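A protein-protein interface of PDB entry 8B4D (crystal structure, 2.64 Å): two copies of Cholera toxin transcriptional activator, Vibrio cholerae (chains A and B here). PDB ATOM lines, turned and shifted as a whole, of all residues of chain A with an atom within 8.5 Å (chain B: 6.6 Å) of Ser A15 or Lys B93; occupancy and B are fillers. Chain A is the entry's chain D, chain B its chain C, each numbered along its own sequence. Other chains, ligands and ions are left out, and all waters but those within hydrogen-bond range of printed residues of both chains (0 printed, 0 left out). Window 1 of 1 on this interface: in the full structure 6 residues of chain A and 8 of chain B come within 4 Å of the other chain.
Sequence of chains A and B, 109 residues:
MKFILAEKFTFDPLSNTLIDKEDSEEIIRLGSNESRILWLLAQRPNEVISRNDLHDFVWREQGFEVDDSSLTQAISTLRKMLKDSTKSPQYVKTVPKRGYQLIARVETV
The side-chain amide oxygen (OD1) of Asn B46 is in hydrogen-bond range of the side-chain hydroxyl (OG) of Ser A15, at 3.3 Å.
The backbone carbonyl oxygen (O) of Leu A14 lies within hydrogen-bond range of the side-chain amide nitrogen (NE2) of Gln B101 (3.3 Å).
Of the 18 printed residues of chain A, 4 touch a printed residue of chain B.
Hydrophobic or aromatic side chains of chain A that line the printed part of chain B: Leu A14.
Along chain A the printed residues that touch a printed residue of chain B span positions 14 to 32.
Printed residues of chain B that touch a printed residue of chain A: Asn B46, Pro B89, Lys B93, Val B95 and Gln B101.
Hydrophobic or aromatic side chains of chain B that line the printed part of chain A: Pro B89 and Val B95.
Among the printed residues, pairs that only touch across the chains: Ser A32 with Val B95 (3.3 Å), Ser A15 with Lys B93 (3.5 Å), Arg A29 with Pro B89 (3.7 Å) and Leu A14 with Asn B46 (3.9 Å).
No position is printed for both chains.
Of the 6 pairs that touch across the chains among the printed residues, none has its exchanged pair printed and touching as well.
The side-chain amide oxygen of Asn B46 sits at hydrogen-bond distance from the side-chain amide nitrogen of Gln B101 (2.9 Å).
The backbone NH (N) of Asn B46 sits at hydrogen-bond distance from the backbone carbonyl oxygen (O) of Leu B102 (2.9 Å).
The backbone carbonyl oxygen (O) of Gln B101 is in hydrogen-bond range of the backbone NH (N) of Lys B93 (2.8 Å).
The side-chain carboxylate of Asp A12 is in hydrogen-bond range of the side-chain hydroxyl of Ser A15, at 3.1 Å.
The side-chain amide oxygen (OD1) of Asn A16 sits close to the backbone carbonyl oxygen (O) of Leu A14, 3.0 Å away.
Of the printed residues of chain B, Leu A14 touches Asn B46 and Gln B101.
Ser A15 touches just these residues of chain B: Asn B46 and Lys B93.
Of the printed residues of chain B, Ser A32 touches Val B95 (3.3 Å).
Ser A35 touches none of the printed residues of chain B.
Lys B93 touches just one residue of chain A: Ser A15.
Of the printed residues of chain A, Gln B101 touches Leu A14.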
ATOM      1  N   MET A   1      -5.129 -22.022   6.239  1.00  0.00           N
ATOM      2  CA  MET A   1      -5.154 -20.767   5.494  1.00  0.00           C
ATOM      3  C   MET A   1      -6.582 -20.241   5.334  1.00  0.00           C
ATOM      4  O   MET A   1      -7.385 -20.866   4.640  1.00  0.00           O
ATOM      5  CB  MET A   1      -4.500 -20.968   4.125  1.00  0.00           C
ATOM      6  CG  MET A   1      -4.349 -19.710   3.301  1.00  0.00           C
ATOM      7  SD  MET A   1      -2.700 -19.511   2.592  1.00  0.00           S
ATOM      8  CE  MET A   1      -2.796 -20.582   1.155  1.00  0.00           C
ATOM      9  N   LYS A   2      -6.914 -19.114   5.967  1.00  0.00           N
ATOM     10  CA  LYS A   2      -8.253 -18.545   5.838  1.00  0.00           C
ATOM     11  C   LYS A   2      -8.333 -17.664   4.593  1.00  0.00           C
ATOM     12  O   LYS A   2      -7.320 -17.155   4.100  1.00  0.00           O
ATOM     13  CB  LYS A   2      -8.634 -17.727   7.076  1.00  0.00           C
ATOM     14  CG  LYS A   2      -9.399 -18.488   8.147  1.00  0.00           C
ATOM     15  CD  LYS A   2      -9.140 -17.909   9.532  1.00  0.00           C
ATOM     16  CE  LYS A   2     -10.076 -18.508  10.583  1.00  0.00           C
ATOM     17  NZ  LYS A   2      -9.532 -18.469  11.969  1.00  0.00           N
ATOM     18  N   PHE A  11     -13.883 -17.568   4.789  1.00  0.00           N
ATOM     19  CA  PHE A  11     -13.927 -18.988   4.455  1.00  0.00           C
ATOM     20  C   PHE A  11     -12.754 -19.683   5.122  1.00  0.00           C
ATOM     21  O   PHE A  11     -11.593 -19.341   4.863  1.00  0.00           O
ATOM     22  CB  PHE A  11     -13.863 -19.210   2.937  1.00  0.00           C
ATOM     23  CG  PHE A  11     -13.728 -20.667   2.521  1.00  0.00           C
ATOM     24  CD1 PHE A  11     -14.459 -21.664   3.143  1.00  0.00           C
ATOM     25  CD2 PHE A  11     -12.874 -21.026   1.494  1.00  0.00           C
ATOM     26  CE1 PHE A  11     -14.322 -22.989   2.754  1.00  0.00           C
ATOM     27  CE2 PHE A  11     -12.744 -22.365   1.089  1.00  0.00           C
ATOM     28  CZ  PHE A  11     -13.458 -23.334   1.720  1.00  0.00           C
ATOM     29  N   ASP A  12     -13.052 -20.661   5.970  1.00  0.00           N
ATOM     30  CA  ASP A  12     -12.005 -21.467   6.584  1.00  0.00           C
ATOM     31  C   ASP A  12     -12.015 -22.869   5.982  1.00  0.00           C
ATOM     32  O   ASP A  12     -12.909 -23.669   6.301  1.00  0.00           O
ATOM     33  CB  ASP A  12     -12.222 -21.518   8.094  1.00  0.00           C
ATOM     34  CG  ASP A  12     -11.082 -22.174   8.804  1.00  0.00           C
ATOM     35  OD1 ASP A  12     -10.006 -22.282   8.182  1.00  0.00           O
ATOM     36  OD2 ASP A  12     -11.239 -22.545   9.986  1.00  0.00           O
ATOM     37  N   PRO A  13     -11.076 -23.211   5.085  1.00  0.00           N
ATOM     38  CA  PRO A  13     -11.192 -24.484   4.352  1.00  0.00           C
ATOM     39  C   PRO A  13     -10.935 -25.711   5.206  1.00  0.00           C
ATOM     40  O   PRO A  13     -11.335 -26.816   4.813  1.00  0.00           O
ATOM     41  CB  PRO A  13     -10.156 -24.331   3.230  1.00  0.00           C
ATOM     42  CG  PRO A  13      -9.174 -23.411   3.786  1.00  0.00           C
ATOM     43  CD  PRO A  13      -9.999 -22.390   4.523  1.00  0.00           C
ATOM     44  N   LEU A  14     -10.329 -25.538   6.379  1.00  0.00           N
ATOM     45  CA  LEU A  14      -9.975 -26.630   7.260  1.00  0.00           C
ATOM     46  C   LEU A  14     -11.124 -26.937   8.204  1.00  0.00           C
ATOM     47  O   LEU A  14     -11.589 -28.063   8.276  1.00  0.00           O
ATOM     48  CB  LEU A  14      -8.707 -26.270   8.037  1.00  0.00           C
ATOM     49  CG  LEU A  14      -7.506 -25.727   7.208  1.00  0.00           C
ATOM     50  CD1 LEU A  14      -6.311 -25.503   8.104  1.00  0.00           C
ATOM     51  CD2 LEU A  14      -7.113 -26.582   5.986  1.00  0.00           C
ATOM     52  N   SER A  15     -11.622 -25.953   8.930  1.00  0.00           N
ATOM     53  CA  SER A  15     -12.784 -26.193   9.778  1.00  0.00           C
ATOM     54  C   SER A  15     -14.051 -26.367   8.958  1.00  0.00           C
ATOM     55  O   SER A  15     -14.997 -26.990   9.442  1.00  0.00           O
ATOM     56  CB  SER A  15     -12.941 -25.038  10.781  1.00  0.00           C
ATOM     57  OG  SER A  15     -11.826 -25.031  11.664  1.00  0.00           O
ATOM     58  N   ASN A  16     -14.065 -25.834   7.723  1.00  0.00           N
ATOM     59  CA  ASN A  16     -15.188 -25.869   6.778  1.00  0.00           C
ATOM     60  C   ASN A  16     -16.307 -24.915   7.168  1.00  0.00           C
ATOM     61  O   ASN A  16     -17.483 -25.247   7.059  1.00  0.00           O
ATOM     62  CB  ASN A  16     -15.718 -27.286   6.582  1.00  0.00           C
ATOM     63  CG  ASN A  16     -14.719 -28.174   5.921  1.00  0.00           C
ATOM     64  OD1 ASN A  16     -13.523 -27.899   5.942  1.00  0.00           O
ATOM     65  ND2 ASN A  16     -15.188 -29.276   5.367  1.00  0.00           N
ATOM     66  N   THR A  17     -15.925 -23.696   7.558  1.00  0.00           N
ATOM     67  CA  THR A  17     -16.847 -22.700   8.095  1.00  0.00           C
ATOM     68  C   THR A  17     -16.899 -21.453   7.211  1.00  0.00           C
ATOM     69  O   THR A  17     -15.937 -21.104   6.521  1.00  0.00           O
ATOM     70  CB  THR A  17     -16.464 -22.282   9.503  1.00  0.00           C
ATOM     71  OG1 THR A  17     -15.297 -21.454   9.447  1.00  0.00           O
ATOM     72  CG2 THR A  17     -16.164 -23.492  10.337  1.00  0.00           C
ATOM     73  N   LEU A  18     -18.041 -20.774   7.262  1.00  0.00           N
ATOM     74  CA  LEU A  18     -18.288 -19.539   6.526  1.00  0.00           C
ATOM     75  C   LEU A  18     -18.931 -18.549   7.493  1.00  0.00           C
ATOM     76  O   LEU A  18     -20.027 -18.811   7.995  1.00  0.00           O
ATOM     77  CB  LEU A  18     -19.182 -19.829   5.318  1.00  0.00           C
ATOM     78  CG  LEU A  18     -18.681 -19.798   3.879  1.00  0.00           C
ATOM     79  CD1 LEU A  18     -19.870 -19.612   2.966  1.00  0.00           C
ATOM     80  CD2 LEU A  18     -17.630 -18.716   3.631  1.00  0.00           C
ATOM     81  N   ILE A  19     -18.239 -17.446   7.784  1.00  0.00           N
ATOM     82  CA  ILE A  19     -18.812 -16.353   8.569  1.00  0.00           C
ATOM     83  C   ILE A  19     -19.106 -15.205   7.629  1.00  0.00           C
ATOM     84  O   ILE A  19     -18.188 -14.657   7.008  1.00  0.00           O
ATOM     85  CB  ILE A  19     -17.904 -15.889   9.711  1.00  0.00           C
ATOM     86  CG1 ILE A  19     -17.658 -17.038  10.676  1.00  0.00           C
ATOM     87  CG2 ILE A  19     -18.543 -14.750  10.466  1.00  0.00           C
ATOM     88  CD1 ILE A  19     -16.266 -17.565  10.614  1.00  0.00           C
ATOM     89  N   ILE A  27     -22.104 -19.250  12.512  1.00  0.00           N
ATOM     90  CA  ILE A  27     -21.178 -20.025  11.689  1.00  0.00           C
ATOM     91  C   ILE A  27     -21.998 -20.743  10.635  1.00  0.00           C
ATOM     92  O   ILE A  27     -23.013 -21.376  10.956  1.00  0.00           O
ATOM     93  CB  ILE A  27     -20.346 -21.023  12.510  1.00  0.00           C
ATOM     94  CG1 ILE A  27     -19.697 -20.351  13.724  1.00  0.00           C
ATOM     95  CG2 ILE A  27     -19.265 -21.584  11.629  1.00  0.00           C
ATOM     96  CD1 ILE A  27     -18.988 -19.034  13.420  1.00  0.00           C
ATOM     97  N   ILE A  28     -21.594 -20.599   9.376  1.00  0.00           N
ATOM     98  CA  ILE A  28     -22.220 -21.347   8.288  1.00  0.00           C
ATOM     99  C   ILE A  28     -21.381 -22.589   8.024  1.00  0.00           C
ATOM    100  O   ILE A  28     -20.204 -22.498   7.650  1.00  0.00           O
ATOM    101  CB  ILE A  28     -22.381 -20.496   7.018  1.00  0.00           C
ATOM    102  CG1 ILE A  28     -23.121 -19.184   7.338  1.00  0.00           C
ATOM    103  CG2 ILE A  28     -23.076 -21.308   5.934  1.00  0.00           C
ATOM    104  CD1 ILE A  28     -23.462 -18.366   6.138  1.00  0.00           C
ATOM    105  N   ARG A  29     -21.982 -23.750   8.237  1.00  0.00           N
ATOM    106  CA  ARG A  29     -21.293 -25.026   8.096  1.00  0.00           C
ATOM    107  C   ARG A  29     -21.575 -25.609   6.718  1.00  0.00           C
ATOM    108  O   ARG A  29     -22.716 -25.971   6.404  1.00  0.00           O
ATOM    109  CB  ARG A  29     -21.726 -25.965   9.202  1.00  0.00           C
ATOM    110  CG  ARG A  29     -21.529 -25.309  10.518  1.00  0.00           C
ATOM    111  CD  ARG A  29     -21.212 -26.305  11.574  1.00  0.00           C
ATOM    112  NE  ARG A  29     -20.867 -25.605  12.796  1.00  0.00           N
ATOM    113  CZ  ARG A  29     -21.724 -24.885  13.500  1.00  0.00           C
ATOM    114  NH1 ARG A  29     -22.995 -24.772  13.136  1.00  0.00           N
ATOM    115  NH2 ARG A  29     -21.298 -24.272  14.602  1.00  0.00           N
ATOM    116  N   LEU A  30     -20.532 -25.653   5.895  1.00  0.00           N
ATOM    117  CA  LEU A  30     -20.559 -26.241   4.566  1.00  0.00           C
ATOM    118  C   LEU A  30     -20.329 -27.742   4.655  1.00  0.00           C
ATOM    119  O   LEU A  30     -19.563 -28.221   5.496  1.00  0.00           O
ATOM    120  CB  LEU A  30     -19.427 -25.648   3.727  1.00  0.00           C
ATOM    121  CG  LEU A  30     -19.304 -24.136   3.581  1.00  0.00           C
ATOM    122  CD1 LEU A  30     -18.094 -23.893   2.708  1.00  0.00           C
ATOM    123  CD2 LEU A  30     -20.604 -23.537   3.002  1.00  0.00           C
ATOM    124  N   GLY A  31     -20.930 -28.492   3.740  1.00  0.00           N
ATOM    125  CA  GLY A  31     -20.503 -29.867   3.562  1.00  0.00           C
ATOM    126  C   GLY A  31     -19.054 -29.939   3.124  1.00  0.00           C
ATOM    127  O   GLY A  31     -18.482 -28.959   2.637  1.00  0.00           O
ATOM    128  N   SER A  32     -18.450 -31.120   3.287  1.00  0.00           N
ATOM    129  CA  SER A  32     -17.105 -31.343   2.763  1.00  0.00           C
ATOM    130  C   SER A  32     -17.028 -30.986   1.291  1.00  0.00           C
ATOM    131  O   SER A  32     -16.208 -30.161   0.877  1.00  0.00           O
ATOM    132  CB  SER A  32     -16.682 -32.792   2.961  1.00  0.00           C
ATOM    133  OG  SER A  32     -16.052 -32.977   4.218  1.00  0.00           O
ATOM    134  N   SER A  35     -17.292 -27.387   0.669  1.00  0.00           N
ATOM    135  CA  SER A  35     -16.061 -26.759   1.127  1.00  0.00           C
ATOM    136  C   SER A  35     -14.920 -26.966   0.139  1.00  0.00           C
ATOM    137  O   SER A  35     -14.206 -26.016  -0.185  1.00  0.00           O
ATOM    138  CB  SER A  35     -15.691 -27.298   2.492  1.00  0.00           C
ATOM    139  OG  SER A  35     -14.822 -26.392   3.134  1.00  0.00           O
ATOM    140  N   LEU B  41      -6.463 -36.945  18.493  1.00  0.00           N
ATOM    141  CA  LEU B  41      -7.076 -35.774  17.859  1.00  0.00           C
ATOM    142  C   LEU B  41      -6.268 -34.502  18.145  1.00  0.00           C
ATOM    143  O   LEU B  41      -6.005 -33.705  17.237  1.00  0.00           O
ATOM    144  CB  LEU B  41      -8.536 -35.609  18.314  1.00  0.00           C
ATOM    145  CG  LEU B  41      -9.626 -36.479  17.668  1.00  0.00           C
ATOM    146  CD1 LEU B  41     -10.992 -36.153  18.208  1.00  0.00           C
ATOM    147  CD2 LEU B  41      -9.625 -36.300  16.156  1.00  0.00           C
ATOM    148  N   ASN B  46      -6.943 -29.725  14.227  1.00  0.00           N
ATOM    149  CA  ASN B  46      -7.661 -29.271  13.051  1.00  0.00           C
ATOM    150  C   ASN B  46      -7.374 -30.137  11.817  1.00  0.00           C
ATOM    151  O   ASN B  46      -7.547 -29.673  10.689  1.00  0.00           O
ATOM    152  CB  ASN B  46      -7.346 -27.799  12.777  1.00  0.00           C
ATOM    153  CG  ASN B  46      -8.567 -27.011  12.298  1.00  0.00           C
ATOM    154  OD1 ASN B  46      -9.715 -27.493  12.337  1.00  0.00           O
ATOM    155  ND2 ASN B  46      -8.324 -25.780  11.852  1.00  0.00           N
ATOM    156  N   VAL B  48      -8.254 -33.945   9.903  1.00  0.00           N
ATOM    157  CA  VAL B  48      -9.283 -34.982   9.850  1.00  0.00           C
ATOM    158  C   VAL B  48      -8.612 -36.360   9.948  1.00  0.00           C
ATOM    159  O   VAL B  48      -7.815 -36.742   9.083  1.00  0.00           O
ATOM    160  CB  VAL B  48     -10.132 -34.845   8.579  1.00  0.00           C
ATOM    161  CG1 VAL B  48     -10.990 -36.074   8.374  1.00  0.00           C
ATOM    162  CG2 VAL B  48     -11.027 -33.599   8.680  1.00  0.00           C
ATOM    163  N   ARG B  79     -18.033 -36.531  23.164  1.00  0.00           N
ATOM    164  CA  ARG B  79     -18.831 -35.319  22.976  1.00  0.00           C
ATOM    165  C   ARG B  79     -19.717 -35.041  24.187  1.00  0.00           C
ATOM    166  O   ARG B  79     -19.823 -33.892  24.651  1.00  0.00           O
ATOM    167  CB  ARG B  79     -19.679 -35.461  21.726  1.00  0.00           C
ATOM    168  CG  ARG B  79     -18.962 -35.082  20.470  1.00  0.00           C
ATOM    169  CD  ARG B  79     -19.946 -34.936  19.350  1.00  0.00           C
ATOM    170  NE  ARG B  79     -19.268 -34.668  18.091  1.00  0.00           N
ATOM    171  CZ  ARG B  79     -19.372 -35.466  17.036  1.00  0.00           C
ATOM    172  NH1 ARG B  79     -20.075 -36.591  17.094  1.00  0.00           N
ATOM    173  NH2 ARG B  79     -18.768 -35.122  15.896  1.00  0.00           N
ATOM    174  N   ASP B  84     -20.224 -31.026  23.927  1.00  0.00           N
ATOM    175  CA  ASP B  84     -20.302 -30.674  22.514  1.00  0.00           C
ATOM    176  C   ASP B  84     -21.702 -31.016  22.019  1.00  0.00           C
ATOM    177  O   ASP B  84     -22.463 -31.716  22.688  1.00  0.00           O
ATOM    178  CB  ASP B  84     -19.244 -31.443  21.709  1.00  0.00           C
ATOM    179  CG  ASP B  84     -18.923 -30.807  20.362  1.00  0.00           C
ATOM    180  OD1 ASP B  84     -18.598 -29.604  20.327  1.00  0.00           O
ATOM    181  OD2 ASP B  84     -18.967 -31.522  19.332  1.00  0.00           O
ATOM    182  N   PRO B  89     -21.299 -28.233  16.246  1.00  0.00           N
ATOM    183  CA  PRO B  89     -20.096 -28.675  16.956  1.00  0.00           C
ATOM    184  C   PRO B  89     -19.131 -27.529  17.221  1.00  0.00           C
ATOM    185  O   PRO B  89     -18.989 -26.608  16.410  1.00  0.00           O
ATOM    186  CB  PRO B  89     -19.467 -29.711  16.014  1.00  0.00           C
ATOM    187  CG  PRO B  89     -20.137 -29.584  14.737  1.00  0.00           C
ATOM    188  CD  PRO B  89     -21.343 -28.724  14.870  1.00  0.00           C
ATOM    189  N   GLN B  90     -18.458 -27.602  18.382  1.00  0.00           N
ATOM    190  CA  GLN B  90     -17.364 -26.710  18.715  1.00  0.00           C
ATOM    191  C   GLN B  90     -16.077 -27.429  19.062  1.00  0.00           C
ATOM    192  O   GLN B  90     -15.024 -26.793  19.015  1.00  0.00           O
ATOM    193  CB  GLN B  90     -17.744 -25.802  19.894  1.00  0.00           C
ATOM    194  CG  GLN B  90     -18.893 -24.873  19.632  1.00  0.00           C
ATOM    195  CD  GLN B  90     -19.805 -24.764  20.820  1.00  0.00           C
ATOM    196  OE1 GLN B  90     -20.781 -25.507  20.943  1.00  0.00           O
ATOM    197  NE2 GLN B  90     -19.488 -23.847  21.721  1.00  0.00           N
ATOM    198  N   TYR B  91     -16.116 -28.722  19.398  1.00  0.00           N
ATOM    199  CA  TYR B  91     -14.904 -29.447  19.781  1.00  0.00           C
ATOM    200  C   TYR B  91     -14.565 -30.543  18.781  1.00  0.00           C
ATOM    201  O   TYR B  91     -13.520 -30.482  18.130  1.00  0.00           O
ATOM    202  CB  TYR B  91     -15.059 -30.000  21.201  1.00  0.00           C
ATOM    203  CG  TYR B  91     -15.477 -28.966  22.238  1.00  0.00           C
ATOM    204  CD1 TYR B  91     -14.541 -28.199  22.929  1.00  0.00           C
ATOM    205  CD2 TYR B  91     -16.821 -28.761  22.518  1.00  0.00           C
ATOM    206  CE1 TYR B  91     -14.953 -27.256  23.871  1.00  0.00           C
ATOM    207  CE2 TYR B  91     -17.237 -27.831  23.440  1.00  0.00           C
ATOM    208  CZ  TYR B  91     -16.308 -27.080  24.116  1.00  0.00           C
ATOM    209  OH  TYR B  91     -16.759 -26.157  25.035  1.00  0.00           O
ATOM    210  N   VAL B  92     -15.410 -31.564  18.640  1.00  0.00           N
ATOM    211  CA  VAL B  92     -15.148 -32.711  17.775  1.00  0.00           C
ATOM    212  C   VAL B  92     -16.141 -32.652  16.630  1.00  0.00           C
ATOM    213  O   VAL B  92     -17.354 -32.597  16.863  1.00  0.00           O
ATOM    214  CB  VAL B  92     -15.269 -34.049  18.537  1.00  0.00           C
ATOM    215  CG1 VAL B  92     -15.302 -35.219  17.569  1.00  0.00           C
ATOM    216  CG2 VAL B  92     -14.122 -34.231  19.569  1.00  0.00           C
ATOM    217  N   LYS B  93     -15.631 -32.680  15.403  1.00  0.00           N
ATOM    218  CA  LYS B  93     -16.430 -32.537  14.195  1.00  0.00           C
ATOM    219  C   LYS B  93     -16.369 -33.820  13.372  1.00  0.00           C
ATOM    220  O   LYS B  93     -15.357 -34.527  13.392  1.00  0.00           O
ATOM    221  CB  LYS B  93     -15.920 -31.339  13.377  1.00  0.00           C
ATOM    222  CG  LYS B  93     -15.990 -31.493  11.868  1.00  0.00           C
ATOM    223  CD  LYS B  93     -16.233 -30.173  11.171  1.00  0.00           C
ATOM    224  CE  LYS B  93     -15.989 -30.307   9.697  1.00  0.00           C
ATOM    225  NZ  LYS B  93     -14.540 -30.581   9.435  1.00  0.00           N
ATOM    226  N   THR B  94     -17.451 -34.125  12.655  1.00  0.00           N
ATOM    227  CA  THR B  94     -17.558 -35.341  11.853  1.00  0.00           C
ATOM    228  C   THR B  94     -17.424 -35.054  10.357  1.00  0.00           C
ATOM    229  O   THR B  94     -18.029 -34.120   9.821  1.00  0.00           O
ATOM    230  CB  THR B  94     -18.892 -36.061  12.118  1.00  0.00           C
ATOM    231  OG1 THR B  94     -19.008 -36.377  13.516  1.00  0.00           O
ATOM    232  CG2 THR B  94     -18.994 -37.342  11.309  1.00  0.00           C
ATOM    233  N   VAL B  95     -16.659 -35.885   9.670  1.00  0.00           N
ATOM    234  CA  VAL B  95     -16.468 -35.658   8.243  1.00  0.00           C
ATOM    235  C   VAL B  95     -16.805 -36.966   7.544  1.00  0.00           C
ATOM    236  O   VAL B  95     -15.929 -37.827   7.389  1.00  0.00           O
ATOM    237  CB  VAL B  95     -15.036 -35.187   7.940  1.00  0.00           C
ATOM    238  CG1 VAL B  95     -14.821 -35.144   6.438  1.00  0.00           C
ATOM    239  CG2 VAL B  95     -14.748 -33.838   8.633  1.00  0.00           C
ATOM    240  N   GLY B  99     -13.655 -39.495   8.593  1.00  0.00           N
ATOM    241  CA  GLY B  99     -13.220 -39.619   9.970  1.00  0.00           C
ATOM    242  C   GLY B  99     -13.702 -38.492  10.864  1.00  0.00           C
ATOM    243  O   GLY B  99     -14.764 -37.907  10.603  1.00  0.00           O
ATOM    244  N   TYR B 100     -12.935 -38.182  11.917  1.00  0.00           N
ATOM    245  CA  TYR B 100     -13.260 -37.144  12.882  1.00  0.00           C
ATOM    246  C   TYR B 100     -12.144 -36.105  12.954  1.00  0.00           C
ATOM    247  O   TYR B 100     -10.989 -36.367  12.602  1.00  0.00           O
ATOM    248  CB  TYR B 100     -13.524 -37.742  14.265  1.00  0.00           C
ATOM    249  CG  TYR B 100     -14.697 -38.713  14.269  1.00  0.00           C
ATOM    250  CD1 TYR B 100     -16.016 -38.244  14.403  1.00  0.00           C
ATOM    251  CD2 TYR B 100     -14.497 -40.086  14.118  1.00  0.00           C
ATOM    252  CE1 TYR B 100     -17.085 -39.117  14.395  1.00  0.00           C
ATOM    253  CE2 TYR B 100     -15.558 -40.970  14.110  1.00  0.00           C
ATOM    254  CZ  TYR B 100     -16.850 -40.484  14.251  1.00  0.00           C
ATOM    255  OH  TYR B 100     -17.906 -41.362  14.233  1.00  0.00           O
ATOM    256  N   GLN B 101     -12.500 -34.910  13.428  1.00  0.00           N
ATOM    257  CA  GLN B 101     -11.580 -33.785  13.402  1.00  0.00           C
ATOM    258  C   GLN B 101     -11.782 -32.878  14.600  1.00  0.00           C
ATOM    259  O   GLN B 101     -12.903 -32.435  14.860  1.00  0.00           O
ATOM    260  CB  GLN B 101     -11.760 -32.980  12.130  1.00  0.00           C
ATOM    261  CG  GLN B 101     -11.048 -31.656  12.198  1.00  0.00           C
ATOM    262  CD  GLN B 101     -11.343 -30.773  11.021  1.00  0.00           C
ATOM    263  OE1 GLN B 101     -12.346 -30.950  10.323  1.00  0.00           O
ATOM    264  NE2 GLN B 101     -10.479 -29.793  10.804  1.00  0.00           N
ATOM    265  N   LEU B 102     -10.684 -32.568  15.286  1.00  0.00           N
ATOM    266  CA  LEU B 102     -10.686 -31.697  16.463  1.00  0.00           C
ATOM    267  C   LEU B 102     -10.574 -30.234  16.014  1.00  0.00           C
ATOM    268  O   LEU B 102      -9.482 -29.737  15.694  1.00  0.00           O
ATOM    269  CB  LEU B 102      -9.553 -32.097  17.398  1.00  0.00           C
ATOM    270  CG  LEU B 102      -9.417 -31.330  18.701  1.00  0.00           C
ATOM    271  CD1 LEU B 102     -10.536 -31.650  19.675  1.00  0.00           C
ATOM    272  CD2 LEU B 102      -8.059 -31.656  19.281  1.00  0.00           C
ATOM    273  N   ILE B 103     -11.717 -29.536  15.977  1.00  0.00           N
ATOM    274  CA  ILE B 103     -11.730 -28.166  15.481  1.00  0.00           C
ATOM    275  C   ILE B 103     -11.540 -27.150  16.596  1.00  0.00           C
ATOM    276  O   ILE B 103     -11.476 -25.943  16.316  1.00  0.00           O
ATOM    277  CB  ILE B 103     -13.033 -27.854  14.720  1.00  0.00           C
ATOM    278  CG1 ILE B 103     -14.232 -28.040  15.659  1.00  0.00           C
ATOM    279  CG2 ILE B 103     -13.088 -28.700  13.468  1.00  0.00           C
ATOM    280  CD1 ILE B 103     -15.575 -27.855  15.043  1.00  0.00           C
